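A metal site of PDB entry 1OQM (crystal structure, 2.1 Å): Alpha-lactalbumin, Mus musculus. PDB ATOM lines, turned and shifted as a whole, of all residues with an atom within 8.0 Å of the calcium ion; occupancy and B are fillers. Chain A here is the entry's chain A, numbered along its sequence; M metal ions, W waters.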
ATOM      1  N   THR A  38      15.981  30.925   8.084  1.00  0.00           N
ATOM      2  CA  THR A  38      15.084  30.023   7.377  1.00  0.00           C
ATOM      3  C   THR A  38      15.338  29.948   5.879  1.00  0.00           C
ATOM      4  O   THR A  38      14.821  29.045   5.207  1.00  0.00           O
ATOM      5  CB  THR A  38      13.628  30.440   7.559  1.00  0.00           C
ATOM      6  OG1 THR A  38      13.464  31.761   7.034  1.00  0.00           O
ATOM      7  CG2 THR A  38      13.214  30.402   9.020  1.00  0.00           C
ATOM      8  N   ILE A  75       9.552  16.081  -0.668  1.00  0.00           N
ATOM      9  CA  ILE A  75       9.238  17.496  -0.626  1.00  0.00           C
ATOM     10  C   ILE A  75      10.181  18.281  -1.513  1.00  0.00           C
ATOM     11  O   ILE A  75      11.331  17.897  -1.700  1.00  0.00           O
ATOM     12  CB  ILE A  75       9.369  18.011   0.817  1.00  0.00           C
ATOM     13  CG1 ILE A  75       8.640  19.338   0.971  1.00  0.00           C
ATOM     14  CG2 ILE A  75      10.855  18.131   1.218  1.00  0.00           C
ATOM     15  CD1 ILE A  75       8.517  19.769   2.406  1.00  0.00           C
ATOM     16  N   SER A  76       9.689  19.378  -2.068  1.00  0.00           N
ATOM     17  CA  SER A  76      10.518  20.231  -2.903  1.00  0.00           C
ATOM     18  C   SER A  76      11.427  20.956  -1.933  1.00  0.00           C
ATOM     19  O   SER A  76      10.940  21.398  -0.883  1.00  0.00           O
ATOM     20  CB  SER A  76       9.684  21.285  -3.635  1.00  0.00           C
ATOM     21  OG  SER A  76      10.532  22.268  -4.207  1.00  0.00           O
ATOM     22  N   CYS A  77      12.709  21.080  -2.258  1.00  0.00           N
ATOM     23  CA  CYS A  77      13.633  21.794  -1.362  1.00  0.00           C
ATOM     24  C   CYS A  77      13.192  23.245  -1.146  1.00  0.00           C
ATOM     25  O   CYS A  77      13.473  23.817  -0.097  1.00  0.00           O
ATOM     26  CB  CYS A  77      15.062  21.783  -1.906  1.00  0.00           C
ATOM     27  SG  CYS A  77      15.832  20.153  -2.210  1.00  0.00           S
ATOM     28  N   ASP A  78      12.497  23.836  -2.131  1.00  0.00           N
ATOM     29  CA  ASP A  78      12.063  25.229  -1.972  1.00  0.00           C
ATOM     30  C   ASP A  78      11.093  25.408  -0.822  1.00  0.00           C
ATOM     31  O   ASP A  78      10.926  26.518  -0.315  1.00  0.00           O
ATOM     32  CB  ASP A  78      11.414  25.757  -3.256  1.00  0.00           C
ATOM     33  CG  ASP A  78      12.385  25.825  -4.406  1.00  0.00           C
ATOM     34  OD1 ASP A  78      13.599  25.986  -4.149  1.00  0.00           O
ATOM     35  OD2 ASP A  78      11.920  25.734  -5.575  1.00  0.00           O
ATOM     36  N   LYS A  79      10.453  24.315  -0.414  1.00  0.00           N
ATOM     37  CA  LYS A  79       9.507  24.344   0.696  1.00  0.00           C
ATOM     38  C   LYS A  79      10.282  24.461   2.034  1.00  0.00           C
ATOM     39  O   LYS A  79       9.695  24.705   3.107  1.00  0.00           O
ATOM     40  CB  LYS A  79       8.683  23.055   0.703  1.00  0.00           C
ATOM     41  CG  LYS A  79       7.595  22.968  -0.369  1.00  0.00           C
ATOM     42  CD  LYS A  79       6.416  23.909  -0.057  1.00  0.00           C
ATOM     43  CE  LYS A  79       5.219  23.576  -0.946  1.00  0.00           C
ATOM     44  NZ  LYS A  79       4.039  24.376  -0.564  1.00  0.00           N
ATOM     45  N   LEU A  80      11.592  24.296   1.954  1.00  0.00           N
ATOM     46  CA  LEU A  80      12.434  24.396   3.144  1.00  0.00           C
ATOM     47  C   LEU A  80      13.053  25.793   3.270  1.00  0.00           C
ATOM     48  O   LEU A  80      13.880  26.032   4.156  1.00  0.00           O
ATOM     49  CB  LEU A  80      13.561  23.358   3.103  1.00  0.00           C
ATOM     50  CG  LEU A  80      13.094  21.894   3.057  1.00  0.00           C
ATOM     51  CD1 LEU A  80      14.292  20.960   2.998  1.00  0.00           C
ATOM     52  CD2 LEU A  80      12.252  21.614   4.277  1.00  0.00           C
ATOM     53  N   LEU A  81      12.661  26.704   2.372  1.00  0.00           N
ATOM     54  CA  LEU A  81      13.179  28.059   2.392  1.00  0.00           C
ATOM     55  C   LEU A  81      12.162  29.103   2.841  1.00  0.00           C
ATOM     56  O   LEU A  81      12.335  30.284   2.568  1.00  0.00           O
ATOM     57  CB  LEU A  81      13.744  28.428   1.013  1.00  0.00           C
ATOM     58  CG  LEU A  81      15.033  27.701   0.638  1.00  0.00           C
ATOM     59  CD1 LEU A  81      15.515  28.128  -0.757  1.00  0.00           C
ATOM     60  CD2 LEU A  81      16.090  28.004   1.704  1.00  0.00           C
ATOM     61  N   ASP A  82      11.082  28.690   3.517  1.00  0.00           N
ATOM     62  CA  ASP A  82      10.087  29.658   3.967  1.00  0.00           C
ATOM     63  C   ASP A  82      10.008  29.637   5.486  1.00  0.00           C
ATOM     64  O   ASP A  82      10.745  28.907   6.145  1.00  0.00           O
ATOM     65  CB  ASP A  82       8.708  29.344   3.365  1.00  0.00           C
ATOM     66  CG  ASP A  82       8.218  27.941   3.722  1.00  0.00           C
ATOM     67  OD1 ASP A  82       8.333  27.562   4.908  1.00  0.00           O
ATOM     68  OD2 ASP A  82       7.711  27.227   2.821  1.00  0.00           O
ATOM     69  N   ASP A  83       9.107  30.436   6.040  1.00  0.00           N
ATOM     70  CA  ASP A  83       8.940  30.527   7.484  1.00  0.00           C
ATOM     71  C   ASP A  83       7.962  29.539   8.093  1.00  0.00           C
ATOM     72  O   ASP A  83       7.615  29.638   9.268  1.00  0.00           O
ATOM     73  CB  ASP A  83       8.537  31.945   7.865  1.00  0.00           C
ATOM     74  CG  ASP A  83       9.675  32.924   7.712  1.00  0.00           C
ATOM     75  OD1 ASP A  83      10.826  32.472   7.527  1.00  0.00           O
ATOM     76  OD2 ASP A  83       9.429  34.149   7.797  1.00  0.00           O
ATOM     77  N   GLU A  84       7.479  28.592   7.300  1.00  0.00           N
ATOM     78  CA  GLU A  84       6.561  27.574   7.812  1.00  0.00           C
ATOM     79  C   GLU A  84       7.427  26.344   8.049  1.00  0.00           C
ATOM     80  O   GLU A  84       7.834  25.629   7.110  1.00  0.00           O
ATOM     81  CB  GLU A  84       5.418  27.339   6.802  1.00  0.00           C
ATOM     82  CG  GLU A  84       4.324  28.415   6.889  1.00  0.00           C
ATOM     83  CD  GLU A  84       3.588  28.636   5.556  1.00  0.00           C
ATOM     84  OE1 GLU A  84       2.868  27.712   5.059  1.00  0.00           O
ATOM     85  OE2 GLU A  84       3.748  29.746   5.020  1.00  0.00           O
ATOM     86  N   LEU A  85       7.713  26.111   9.324  1.00  0.00           N
ATOM     87  CA  LEU A  85       8.612  25.039   9.758  1.00  0.00           C
ATOM     88  C   LEU A  85       8.072  23.631   9.944  1.00  0.00           C
ATOM     89  O   LEU A  85       8.848  22.724  10.238  1.00  0.00           O
ATOM     90  CB  LEU A  85       9.336  25.495  11.030  1.00  0.00           C
ATOM     91  CG  LEU A  85      10.638  26.299  10.971  1.00  0.00           C
ATOM     92  CD1 LEU A  85      10.956  26.864   9.593  1.00  0.00           C
ATOM     93  CD2 LEU A  85      10.562  27.376  12.010  1.00  0.00           C
ATOM     94  N   ASP A  86       6.763  23.429   9.796  1.00  0.00           N
ATOM     95  CA  ASP A  86       6.206  22.086   9.973  1.00  0.00           C
ATOM     96  C   ASP A  86       6.771  21.081   8.975  1.00  0.00           C
ATOM     97  O   ASP A  86       7.068  19.937   9.337  1.00  0.00           O
ATOM     98  CB  ASP A  86       4.678  22.105   9.898  1.00  0.00           C
ATOM     99  CG  ASP A  86       4.051  22.873  11.045  1.00  0.00           C
ATOM    100  OD1 ASP A  86       4.407  24.053  11.233  1.00  0.00           O
ATOM    101  OD2 ASP A  86       3.179  22.314  11.754  1.00  0.00           O
ATOM    102  N   ASP A  87       6.947  21.479   7.704  1.00  0.00           N
ATOM    103  CA  ASP A  87       7.494  20.496   6.766  1.00  0.00           C
ATOM    104  C   ASP A  87       9.001  20.328   6.972  1.00  0.00           C
ATOM    105  O   ASP A  87       9.528  19.231   6.767  1.00  0.00           O
ATOM    106  CB  ASP A  87       7.146  20.801   5.285  1.00  0.00           C
ATOM    107  CG  ASP A  87       7.380  22.260   4.872  1.00  0.00           C
ATOM    108  OD1 ASP A  87       8.040  23.021   5.620  1.00  0.00           O
ATOM    109  OD2 ASP A  87       6.893  22.641   3.779  1.00  0.00           O
ATOM    110  N   ASP A  88       9.701  21.384   7.394  1.00  0.00           N
ATOM    111  CA  ASP A  88      11.143  21.263   7.662  1.00  0.00           C
ATOM    112  C   ASP A  88      11.352  20.256   8.822  1.00  0.00           C
ATOM    113  O   ASP A  88      12.215  19.399   8.780  1.00  0.00           O
ATOM    114  CB  ASP A  88      11.766  22.590   8.080  1.00  0.00           C
ATOM    115  CG  ASP A  88      11.550  23.696   7.048  1.00  0.00           C
ATOM    116  OD1 ASP A  88      12.523  24.323   6.608  1.00  0.00           O
ATOM    117  OD2 ASP A  88      10.400  23.947   6.689  1.00  0.00           O
ATOM    118  N   ILE A  89      10.541  20.396   9.857  1.00  0.00           N
ATOM    119  CA  ILE A  89      10.604  19.547  11.044  1.00  0.00           C
ATOM    120  C   ILE A  89      10.309  18.086  10.727  1.00  0.00           C
ATOM    121  O   ILE A  89      11.004  17.188  11.185  1.00  0.00           O
ATOM    122  CB  ILE A  89       9.630  20.095  12.131  1.00  0.00           C
ATOM    123  CG1 ILE A  89      10.165  21.441  12.656  1.00  0.00           C
ATOM    124  CG2 ILE A  89       9.451  19.066  13.256  1.00  0.00           C
ATOM    125  CD1 ILE A  89       9.152  22.308  13.413  1.00  0.00           C
HETATM  126 CA    CA M   1       8.899  25.145   5.262  1.00  0.00          CA
HETATM  127  O   HOH W   1       6.845  25.140   4.006  1.00  0.00           O
HETATM  128  O   HOH W   2      11.115  26.436   5.544  1.00  0.00           O
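The calcium ion is bound by O of Glu 84 (2.2 Å).
OD1 of Asp 87 is bound to the calcium ion (2.3 Å).
The calcium ion is bound by the backbone carbonyl oxygen (O) of Lys 79 (2.3 Å).
OD2 of Asp 88 is bound to the calcium ion (2.4 Å).
Water W1 binds the calcium ion, at 2.4 Å.
OD1 of Asp 82 binds the calcium ion (2.5 Å).
Water W2 binds the calcium ion, 2.6 Å away.
The calcium ion has seven donor atoms within binding distance.
Within 4 Å of the calcium ion: Lys 79, Asp 82, Glu 84, Asp 87 and Asp 88.
The nearest printed residue that does not touch the calcium ion is Leu 80 (4.2 Å).
Water W1 lies within hydrogen-bond range of the side-chain carboxylate of Asp 87 (2.5 Å) and the side-chain carboxylate of Asp 82 (2.6 Å).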
